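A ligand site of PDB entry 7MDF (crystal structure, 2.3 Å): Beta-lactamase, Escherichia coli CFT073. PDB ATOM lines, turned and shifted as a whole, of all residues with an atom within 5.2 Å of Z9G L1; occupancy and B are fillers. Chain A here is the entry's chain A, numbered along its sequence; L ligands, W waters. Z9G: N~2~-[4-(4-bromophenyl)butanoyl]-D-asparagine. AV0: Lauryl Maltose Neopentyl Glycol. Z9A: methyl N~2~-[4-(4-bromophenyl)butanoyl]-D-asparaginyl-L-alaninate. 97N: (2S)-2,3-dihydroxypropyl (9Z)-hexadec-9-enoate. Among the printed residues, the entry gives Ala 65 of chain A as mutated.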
ATOM      1  N   GLY A  64     -19.268  13.449  -6.473  1.00  0.00           N
ATOM      2  CA  GLY A  64     -19.692  13.018  -5.157  1.00  0.00           C
ATOM      3  C   GLY A  64     -19.043  13.863  -4.076  1.00  0.00           C
ATOM      4  O   GLY A  64     -18.769  15.058  -4.262  1.00  0.00           O
ATOM      5  N   ALA A  65     -18.740  13.227  -2.955  1.00  0.00           N
ATOM      6  CA  ALA A  65     -18.165  13.920  -1.817  1.00  0.00           C
ATOM      7  C   ALA A  65     -16.750  14.437  -2.086  1.00  0.00           C
ATOM      8  O   ALA A  65     -16.213  15.164  -1.244  1.00  0.00           O
ATOM      9  CB  ALA A  65     -18.174  12.999  -0.613  1.00  0.00           C
ATOM     10  N   LYS A  68     -16.492  18.188  -1.831  1.00  0.00           N
ATOM     11  CA  LYS A  68     -16.338  18.942  -0.579  1.00  0.00           C
ATOM     12  C   LYS A  68     -14.972  19.598  -0.479  1.00  0.00           C
ATOM     13  O   LYS A  68     -14.834  20.648   0.154  1.00  0.00           O
ATOM     14  CB  LYS A  68     -16.564  18.030   0.626  1.00  0.00           C
ATOM     15  CG  LYS A  68     -18.007  17.571   0.767  1.00  0.00           C
ATOM     16  CD  LYS A  68     -18.109  16.543   1.872  1.00  0.00           C
ATOM     17  CE  LYS A  68     -19.539  16.371   2.370  1.00  0.00           C
ATOM     18  NZ  LYS A  68     -20.444  15.702   1.394  1.00  0.00           N
ATOM     19  N   PHE A 122     -28.442  11.943  10.094  1.00  0.00           N
ATOM     20  CA  PHE A 122     -28.207  11.365   8.768  1.00  0.00           C
ATOM     21  C   PHE A 122     -29.315  11.728   7.795  1.00  0.00           C
ATOM     22  O   PHE A 122     -29.060  11.869   6.590  1.00  0.00           O
ATOM     23  CB  PHE A 122     -28.074   9.841   8.891  1.00  0.00           C
ATOM     24  CG  PHE A 122     -27.946   9.134   7.565  1.00  0.00           C
ATOM     25  CD1 PHE A 122     -26.776   9.214   6.835  1.00  0.00           C
ATOM     26  CD2 PHE A 122     -29.011   8.411   7.046  1.00  0.00           C
ATOM     27  CE1 PHE A 122     -26.659   8.591   5.604  1.00  0.00           C
ATOM     28  CE2 PHE A 122     -28.907   7.770   5.819  1.00  0.00           C
ATOM     29  CZ  PHE A 122     -27.727   7.852   5.103  1.00  0.00           C
ATOM     30  N   LEU A 125     -29.512  14.271   4.705  1.00  0.00           N
ATOM     31  CA  LEU A 125     -29.178  13.918   3.332  1.00  0.00           C
ATOM     32  C   LEU A 125     -30.439  13.755   2.482  1.00  0.00           C
ATOM     33  O   LEU A 125     -30.473  14.207   1.332  1.00  0.00           O
ATOM     34  CB  LEU A 125     -28.338  12.634   3.322  1.00  0.00           C
ATOM     35  CG  LEU A 125     -28.065  12.001   1.942  1.00  0.00           C
ATOM     36  CD1 LEU A 125     -27.359  12.969   1.005  1.00  0.00           C
ATOM     37  CD2 LEU A 125     -27.268  10.717   2.069  1.00  0.00           C
ATOM     38  N   GLU A 129     -31.011  16.401  -0.729  1.00  0.00           N
ATOM     39  CA  GLU A 129     -30.875  15.834  -2.071  1.00  0.00           C
ATOM     40  C   GLU A 129     -32.185  15.857  -2.840  1.00  0.00           C
ATOM     41  O   GLU A 129     -32.184  15.668  -4.060  1.00  0.00           O
ATOM     42  CB  GLU A 129     -30.324  14.400  -1.996  1.00  0.00           C
ATOM     43  CG  GLU A 129     -31.378  13.323  -1.778  1.00  0.00           C
ATOM     44  CD  GLU A 129     -30.776  11.936  -1.659  1.00  0.00           C
ATOM     45  OE1 GLU A 129     -29.534  11.802  -1.754  1.00  0.00           O
ATOM     46  OE2 GLU A 129     -31.546  10.970  -1.440  1.00  0.00           O
ATOM     47  N   TYR A 156     -19.938  12.123  10.265  1.00  0.00           N
ATOM     48  CA  TYR A 156     -20.018  12.577   8.878  1.00  0.00           C
ATOM     49  C   TYR A 156     -21.464  12.805   8.452  1.00  0.00           C
ATOM     50  O   TYR A 156     -22.349  11.965   8.699  1.00  0.00           O
ATOM     51  CB  TYR A 156     -19.363  11.545   7.968  1.00  0.00           C
ATOM     52  CG  TYR A 156     -19.126  12.039   6.569  1.00  0.00           C
ATOM     53  CD1 TYR A 156     -20.124  11.956   5.611  1.00  0.00           C
ATOM     54  CD2 TYR A 156     -17.903  12.590   6.216  1.00  0.00           C
ATOM     55  CE1 TYR A 156     -19.911  12.420   4.345  1.00  0.00           C
ATOM     56  CE2 TYR A 156     -17.679  13.034   4.952  1.00  0.00           C
ATOM     57  CZ  TYR A 156     -18.691  12.954   4.011  1.00  0.00           C
ATOM     58  OH  TYR A 156     -18.468  13.401   2.733  1.00  0.00           O
ATOM     59  N   SER A 158     -23.378  14.649   4.883  1.00  0.00           N
ATOM     60  CA  SER A 158     -23.061  15.286   3.607  1.00  0.00           C
ATOM     61  C   SER A 158     -23.545  16.721   3.577  1.00  0.00           C
ATOM     62  O   SER A 158     -22.831  17.612   3.095  1.00  0.00           O
ATOM     63  CB  SER A 158     -23.665  14.469   2.470  1.00  0.00           C
ATOM     64  OG  SER A 158     -23.180  14.965   1.238  1.00  0.00           O
ATOM     65  N   HIS A 227     -27.623  20.995  -3.089  1.00  0.00           N
ATOM     66  CA  HIS A 227     -26.773  19.885  -2.690  1.00  0.00           C
ATOM     67  C   HIS A 227     -25.502  19.813  -3.533  1.00  0.00           C
ATOM     68  O   HIS A 227     -24.610  19.023  -3.211  1.00  0.00           O
ATOM     69  CB  HIS A 227     -27.568  18.590  -2.800  1.00  0.00           C
ATOM     70  CG  HIS A 227     -26.940  17.412  -2.111  1.00  0.00           C
ATOM     71  ND1 HIS A 227     -26.234  17.527  -0.934  1.00  0.00           N
ATOM     72  CD2 HIS A 227     -26.955  16.093  -2.413  1.00  0.00           C
ATOM     73  CE1 HIS A 227     -25.817  16.339  -0.556  1.00  0.00           C
ATOM     74  NE2 HIS A 227     -26.238  15.448  -1.444  1.00  0.00           N
ATOM     75  N   ALA A 230     -21.949  19.654  -1.873  1.00  0.00           N
ATOM     76  CA  ALA A 230     -21.599  18.431  -1.189  1.00  0.00           C
ATOM     77  C   ALA A 230     -21.388  17.246  -2.124  1.00  0.00           C
ATOM     78  O   ALA A 230     -20.745  16.278  -1.713  1.00  0.00           O
ATOM     79  CB  ALA A 230     -22.683  18.051  -0.185  1.00  0.00           C
ATOM     80  N   ALA A 231     -21.908  17.290  -3.345  1.00  0.00           N
ATOM     81  CA  ALA A 231     -22.093  16.040  -4.075  1.00  0.00           C
ATOM     82  C   ALA A 231     -21.944  16.135  -5.596  1.00  0.00           C
ATOM     83  O   ALA A 231     -21.732  15.110  -6.234  1.00  0.00           O
ATOM     84  CB  ALA A 231     -23.475  15.447  -3.769  1.00  0.00           C
ATOM     85  N   TYR A 232     -22.080  17.328  -6.190  1.00  0.00           N
ATOM     86  CA  TYR A 232     -22.403  17.435  -7.604  1.00  0.00           C
ATOM     87  C   TYR A 232     -21.511  18.423  -8.334  1.00  0.00           C
ATOM     88  O   TYR A 232     -21.937  19.019  -9.329  1.00  0.00           O
ATOM     89  CB  TYR A 232     -23.871  17.830  -7.802  1.00  0.00           C
ATOM     90  CG  TYR A 232     -24.860  16.844  -7.245  1.00  0.00           C
ATOM     91  CD1 TYR A 232     -24.743  15.481  -7.527  1.00  0.00           C
ATOM     92  CD2 TYR A 232     -25.914  17.272  -6.435  1.00  0.00           C
ATOM     93  CE1 TYR A 232     -25.676  14.579  -7.013  1.00  0.00           C
ATOM     94  CE2 TYR A 232     -26.838  16.395  -5.930  1.00  0.00           C
ATOM     95  CZ  TYR A 232     -26.717  15.045  -6.216  1.00  0.00           C
ATOM     96  OH  TYR A 232     -27.639  14.182  -5.693  1.00  0.00           O
ATOM     97  N   GLN A 300     -19.220   9.164  -3.165  1.00  0.00           N
ATOM     98  CA  GLN A 300     -20.281   8.175  -3.349  1.00  0.00           C
ATOM     99  C   GLN A 300     -21.607   8.882  -3.621  1.00  0.00           C
ATOM    100  O   GLN A 300     -22.200   9.468  -2.713  1.00  0.00           O
ATOM    101  CB  GLN A 300     -20.386   7.275  -2.130  1.00  0.00           C
ATOM    102  CG  GLN A 300     -21.482   6.258  -2.244  1.00  0.00           C
ATOM    103  CD  GLN A 300     -21.672   5.418  -1.002  1.00  0.00           C
ATOM    104  OE1 GLN A 300     -22.525   4.529  -0.976  1.00  0.00           O
ATOM    105  NE2 GLN A 300     -20.875   5.684   0.043  1.00  0.00           N
ATOM    106  N   ASN A 301     -22.072   8.800  -4.857  1.00  0.00           N
ATOM    107  CA  ASN A 301     -23.371   9.287  -5.282  1.00  0.00           C
ATOM    108  C   ASN A 301     -24.283   8.129  -5.626  1.00  0.00           C
ATOM    109  O   ASN A 301     -23.853   6.983  -5.715  1.00  0.00           O
ATOM    110  CB  ASN A 301     -23.219  10.243  -6.477  1.00  0.00           C
ATOM    111  CG  ASN A 301     -22.852  11.643  -6.020  1.00  0.00           C
ATOM    112  OD1 ASN A 301     -22.601  11.867  -4.845  1.00  0.00           O
ATOM    113  ND2 ASN A 301     -22.792  12.588  -6.951  1.00  0.00           N
ATOM    114  N   PRO A 302     -25.587   8.387  -5.772  1.00  0.00           N
ATOM    115  CA  PRO A 302     -26.498   7.283  -6.094  1.00  0.00           C
ATOM    116  C   PRO A 302     -26.088   6.448  -7.297  1.00  0.00           C
ATOM    117  O   PRO A 302     -26.444   5.261  -7.386  1.00  0.00           O
ATOM    118  CB  PRO A 302     -27.828   8.012  -6.332  1.00  0.00           C
ATOM    119  CG  PRO A 302     -27.756   9.217  -5.412  1.00  0.00           C
ATOM    120  CD  PRO A 302     -26.307   9.636  -5.439  1.00  0.00           C
ATOM    121  N   LEU A 428     -36.462   9.071   7.161  1.00  0.00           N
ATOM    122  CA  LEU A 428     -36.292   8.484   5.840  1.00  0.00           C
ATOM    123  C   LEU A 428     -37.624   8.007   5.298  1.00  0.00           C
ATOM    124  O   LEU A 428     -38.575   7.721   6.050  1.00  0.00           O
ATOM    125  CB  LEU A 428     -35.291   7.318   5.866  1.00  0.00           C
ATOM    126  CG  LEU A 428     -33.876   7.608   6.374  1.00  0.00           C
ATOM    127  CD1 LEU A 428     -32.964   6.397   6.171  1.00  0.00           C
ATOM    128  CD2 LEU A 428     -33.284   8.830   5.695  1.00  0.00           C
ATOM    129  N   PHE A 432     -36.131   8.120  -0.604  1.00  0.00           N
ATOM    130  CA  PHE A 432     -34.702   8.045  -0.314  1.00  0.00           C
ATOM    131  C   PHE A 432     -34.174   6.642  -0.572  1.00  0.00           C
ATOM    132  O   PHE A 432     -33.111   6.466  -1.173  1.00  0.00           O
ATOM    133  CB  PHE A 432     -34.459   8.464   1.138  1.00  0.00           C
ATOM    134  CG  PHE A 432     -33.025   8.367   1.591  1.00  0.00           C
ATOM    135  CD1 PHE A 432     -32.118   9.351   1.261  1.00  0.00           C
ATOM    136  CD2 PHE A 432     -32.608   7.309   2.382  1.00  0.00           C
ATOM    137  CE1 PHE A 432     -30.789   9.272   1.692  1.00  0.00           C
ATOM    138  CE2 PHE A 432     -31.293   7.234   2.830  1.00  0.00           C
ATOM    139  CZ  PHE A 432     -30.385   8.217   2.478  1.00  0.00           C
ATOM    140  N   TRP A 436     -31.145   5.355  -3.511  1.00  0.00           N
ATOM    141  CA  TRP A 436     -29.827   4.810  -3.190  1.00  0.00           C
ATOM    142  C   TRP A 436     -29.707   3.296  -3.342  1.00  0.00           C
ATOM    143  O   TRP A 436     -28.614   2.813  -3.650  1.00  0.00           O
ATOM    144  CB  TRP A 436     -29.444   5.176  -1.757  1.00  0.00           C
ATOM    145  CG  TRP A 436     -29.003   6.582  -1.613  1.00  0.00           C
ATOM    146  CD1 TRP A 436     -29.743   7.626  -1.191  1.00  0.00           C
ATOM    147  CD2 TRP A 436     -27.702   7.095  -1.910  1.00  0.00           C
ATOM    148  NE1 TRP A 436     -28.995   8.778  -1.192  1.00  0.00           N
ATOM    149  CE2 TRP A 436     -27.732   8.469  -1.626  1.00  0.00           C
ATOM    150  CE3 TRP A 436     -26.509   6.521  -2.360  1.00  0.00           C
ATOM    151  CZ2 TRP A 436     -26.617   9.292  -1.796  1.00  0.00           C
ATOM    152  CZ3 TRP A 436     -25.399   7.332  -2.526  1.00  0.00           C
ATOM    153  CH2 TRP A 436     -25.461   8.702  -2.240  1.00  0.00           C
HETATM  154  C13 Z9G L   1     -24.961   7.553   1.275  1.00  0.00           C
HETATM  155  C14 Z9G L   1     -24.831   6.076   1.548  1.00  0.00           C
HETATM  156  C15 Z9G L   1     -26.110   5.448   2.092  1.00  0.00           C
HETATM  157  C16 Z9G L   1     -26.085   4.686   3.245  1.00  0.00           C
HETATM  158  C18 Z9G L   1     -28.435   4.321   3.013  1.00  0.00           C
HETATM  159  C02 Z9G L   1     -23.293   9.447   1.050  1.00  0.00           C
HETATM  160  C04 Z9G L   1     -22.348  11.594   0.270  1.00  0.00           C
HETATM  161  C05 Z9G L   1     -22.435  12.392  -1.014  1.00  0.00           C
HETATM  162  C06 Z9G L   1     -23.841  12.838  -1.389  1.00  0.00           C
HETATM  163  C09 Z9G L   1     -20.966  11.654   0.943  1.00  0.00           C
HETATM  164  C12 Z9G L   1     -23.594   7.977   0.788  1.00  0.00           C
HETATM  165  C17 Z9G L   1     -27.259   4.121   3.714  1.00  0.00           C
HETATM  166  C20 Z9G L   1     -28.452   5.088   1.861  1.00  0.00           C
HETATM  167  C21 Z9G L   1     -27.278   5.653   1.392  1.00  0.00           C
HETATM  168  N03 Z9G L   1     -22.645  10.214   0.002  1.00  0.00           N
HETATM  169  N07 Z9G L   1     -24.500  12.284  -2.564  1.00  0.00           N
HETATM  170  O01 Z9G L   1     -23.579   9.943   2.096  1.00  0.00           O
HETATM  171  O08 Z9G L   1     -24.418  13.631  -0.723  1.00  0.00           O
HETATM  172  O10 Z9G L   1     -20.259  10.613   1.052  1.00  0.00           O
HETATM  173  O11 Z9G L   1     -20.556  12.735   1.425  1.00  0.00           O
HETATM  174 BR19 Z9G L   1     -30.081   3.536   3.618  1.00  0.00          BR
HETATM  175  C1  AV0 L   2     -27.031   4.721   7.901  1.00  0.00           C
HETATM  176  O1  AV0 L   2     -25.669   4.459   7.711  1.00  0.00           O
HETATM  177  C2  AV0 L   2     -27.837   3.434   7.910  1.00  0.00           C
HETATM  178  O2  AV0 L   2     -27.440   2.593   6.810  1.00  0.00           O
HETATM  179  C3  AV0 L   2     -29.267   3.813   7.836  1.00  0.00           C
HETATM  180  O3  AV0 L   2     -30.121   2.618   7.705  1.00  0.00           O
HETATM  181  C4  AV0 L   2     -29.663   4.605   9.041  1.00  0.00           C
HETATM  182  O4  AV0 L   2     -30.981   5.179   8.822  1.00  0.00           O
HETATM  183  C5  AV0 L   2     -28.692   5.742   9.403  1.00  0.00           C
HETATM  184  O5  AV0 L   2     -27.262   5.451   9.169  1.00  0.00           O
HETATM  185  C6  AV0 L   2     -28.881   6.138  10.854  1.00  0.00           C
HETATM  186  O6  AV0 L   2     -27.612   6.330  11.461  1.00  0.00           O
HETATM  187  CAA AV0 L   2     -31.095  10.159  11.093  1.00  0.00           C
HETATM  188  CAW AV0 L   2     -30.463   9.546  12.365  1.00  0.00           C
HETATM  189  CAY AV0 L   2     -29.110  10.238  12.709  1.00  0.00           C
HETATM  190  CAZ AV0 L   2     -17.098   7.547   5.049  1.00  0.00           C
HETATM  191  CBA AV0 L   2     -27.939   9.226  12.619  1.00  0.00           C
HETATM  192  CBB AV0 L   2     -17.447   8.965   4.518  1.00  0.00           C
HETATM  193  CBC AV0 L   2     -26.625   9.927  12.135  1.00  0.00           C
HETATM  194  CBD AV0 L   2     -18.833   8.915   3.803  1.00  0.00           C
HETATM  195  CBE AV0 L   2     -25.715   8.889  11.375  1.00  0.00           C
HETATM  196  CBF AV0 L   2     -19.906   8.312   4.766  1.00  0.00           C
HETATM  197  CBG AV0 L   2     -24.203   9.008  11.823  1.00  0.00           C
HETATM  198  CBH AV0 L   2     -21.144   7.901   3.924  1.00  0.00           C
HETATM  199  CBI AV0 L   2     -23.255   8.577  10.642  1.00  0.00           C
HETATM  200  CBJ AV0 L   2     -22.437   7.967   4.798  1.00  0.00           C
HETATM  201  CBK AV0 L   2     -24.016   7.554   9.709  1.00  0.00           C
HETATM  202  CBL AV0 L   2     -22.703   6.563   5.443  1.00  0.00           C
HETATM  203  CBQ AV0 L   2     -23.250   7.320   8.361  1.00  0.00           C
HETATM  204  CBR AV0 L   2     -23.946   6.005   6.221  1.00  0.00           C
HETATM  205  CBS AV0 L   2     -24.803   5.202   8.591  1.00  0.00           C
HETATM  206  CCM AV0 L   2     -23.592   5.874   7.772  1.00  0.00           C
HETATM  207  C18 Z9A L   3     -24.415   2.238  -0.017  1.00  0.00           C
HETATM  208  C19 Z9A L   3     -25.633   1.381   0.272  1.00  0.00           C
HETATM  209  C20 Z9A L   3     -26.825   2.076  -0.353  1.00  0.00           C
HETATM  210  C21 Z9A L   3     -28.111   1.284  -0.187  1.00  0.00           C
HETATM  211  C22 Z9A L   3     -29.251   1.943   0.265  1.00  0.00           C
HETATM  212  C15 Z9A L   3     -21.251  -5.623   2.081  1.00  0.00           C
HETATM  213  C11 Z9A L   3     -19.277  -2.408   2.189  1.00  0.00           C
HETATM  214  C12 Z9A L   3     -18.060  -2.637   3.091  1.00  0.00           C
HETATM  215  C13 Z9A L   3     -20.335  -3.464   2.443  1.00  0.00           C
HETATM  216  C02 Z9A L   3     -23.252   1.941   0.909  1.00  0.00           C
HETATM  217  C04 Z9A L   3     -20.996   1.028   1.347  1.00  0.00           C
HETATM  218  C05 Z9A L   3     -19.925   2.022   0.931  1.00  0.00           C
HETATM  219  C06 Z9A L   3     -18.930   2.462   1.986  1.00  0.00           C
HETATM  220  C09 Z9A L   3     -20.407  -0.371   1.223  1.00  0.00           C
HETATM  221  C23 Z9A L   3     -30.433   1.233   0.405  1.00  0.00           C
HETATM  222  C24 Z9A L   3     -30.462  -0.120   0.102  1.00  0.00           C
HETATM  223  C26 Z9A L   3     -29.314  -0.774  -0.349  1.00  0.00           C
HETATM  224  C27 Z9A L   3     -28.124  -0.076  -0.493  1.00  0.00           C
HETATM  225  N03 Z9A L   3     -22.076   1.265   0.420  1.00  0.00           N
HETATM  226  N07 Z9A L   3     -17.580   1.937   1.951  1.00  0.00           N
HETATM  227  N10 Z9A L   3     -19.836  -1.065   2.385  1.00  0.00           N
HETATM  228  O01 Z9A L   3     -23.288   2.271   2.051  1.00  0.00           O
HETATM  229  O08 Z9A L   3     -19.264   3.248   2.810  1.00  0.00           O
HETATM  230  O14 Z9A L   3     -20.140  -4.765   1.985  1.00  0.00           O
HETATM  231  O16 Z9A L   3     -21.329  -3.168   3.023  1.00  0.00           O
HETATM  232  O17 Z9A L   3     -20.397  -0.895   0.152  1.00  0.00           O
HETATM  233 BR25 Z9A L   3     -32.119  -1.096   0.294  1.00  0.00          BR
HETATM  234  O   97N L   4     -25.708   0.950   5.415  1.00  0.00           O
HETATM  235  O1  97N L   4     -23.677   0.954   4.466  1.00  0.00           O
HETATM  236  O2  97N L   4     -22.621   3.256   4.960  1.00  0.00           O
HETATM  237  O3  97N L   4     -20.757   3.843   6.701  1.00  0.00           O
HETATM  238  C6  97N L   4     -31.990  -5.595   3.292  1.00  0.00           C
HETATM  239  C7  97N L   4     -31.992  -4.545   4.085  1.00  0.00           C
HETATM  240  C8  97N L   4     -30.659  -3.926   4.537  1.00  0.00           C
HETATM  241  C9  97N L   4     -30.283  -2.735   3.659  1.00  0.00           C
HETATM  242  C10 97N L   4     -29.448  -1.767   4.504  1.00  0.00           C
HETATM  243  C11 97N L   4     -28.984  -0.571   3.677  1.00  0.00           C
HETATM  244  C12 97N L   4     -27.518  -0.716   3.272  1.00  0.00           C
HETATM  245  C13 97N L   4     -26.702  -1.363   4.392  1.00  0.00           C
HETATM  246  C14 97N L   4     -25.225  -1.030   4.195  1.00  0.00           C
HETATM  247  C15 97N L   4     -24.917   0.362   4.751  1.00  0.00           C
HETATM  248  C16 97N L   4     -22.755   0.940   5.523  1.00  0.00           C
HETATM  249  C17 97N L   4     -21.846   2.170   5.380  1.00  0.00           C
HETATM  250  C18 97N L   4     -21.179   2.504   6.718  1.00  0.00           C
HETATM  251  O   HOH W   1     -27.212  12.803  -2.919  1.00  0.00           O
HETATM  252  O   HOH W   2     -23.990  12.002   4.648  1.00  0.00           O
HETATM  253  O   HOH W   3     -17.609   9.581   0.653  1.00  0.00           O
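Water W1 lies within hydrogen-bond range of N07 of Z9G L1, OE1 of Glu 129, OH of Tyr 232 and NE2 of His 227.
Water W2 lies within hydrogen-bond range of N of Ser 158 (2.7 Å) and O01 of Z9G L1 (3.3 Å).
An oxygen (O2) of AV0 L2 sits at hydrogen-bond distance from an oxygen (O) of 97N L4 (2.8 Å).
An oxygen (O01) of Z9A L3 lies within hydrogen-bond range of an oxygen (O2) of 97N L4, 3.1 Å away.
Merely in contact with Z9G L1: Ala 65, Leu 125, Ala 231, Phe 432 and Trp 436.
Hydrophobic or aromatic side chains that line Z9G L1: Ala 65, Leu 125, Tyr 156, His 227, Ala 231, Phe 432 and Trp 436.
Of the 18 residues printed, 11 come within 4 Å of Z9G L1.
The nearest printed residue that does not touch Z9G L1 is Phe 122 (4.01 Å).
NE2 of His 227 sits at hydrogen-bond distance from O08 of Z9G L1, 2.7 Å away.
O of Gln 300 lies within hydrogen-bond range of N03 of Z9G L1, 2.9 Å away.
The side-chain amide oxygen (OD1) of Asn 301 is in hydrogen-bond range of a nitrogen (N07) of Z9G L1 (3.0 Å).
NZ of Lys 68 is in salt-bridge range of O11 of Z9G L1.
OH of Tyr 156 lies within hydrogen-bond range of O11 of Z9G L1 (2.6 Å).
The side-chain hydroxyl (OG) of Ser 158 sits at hydrogen-bond distance from an oxygen (O08) of Z9G L1 (2.7 Å).
The side-chain amino group of Lys 68 lies within hydrogen-bond range of the side-chain hydroxyl of Ser 158.
N of Gly 64 lies within hydrogen-bond range of O of Ala 231.
NE1 of Trp 436 is in hydrogen-bond range of OE1 of Glu 129 (3.1 Å).
The backbone carbonyl oxygen of Ala 230 is in hydrogen-bond range of the side-chain amino group of Lys 68 (3.2 Å).
The side-chain amide nitrogen of Asn 301 sits at hydrogen-bond distance from the backbone carbonyl oxygen of Ala 231 (2.8 Å).
The side-chain amino group (NZ) of Lys 68 sits close to the side-chain hydroxyl (OH) of Tyr 156 (3.3 Å).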
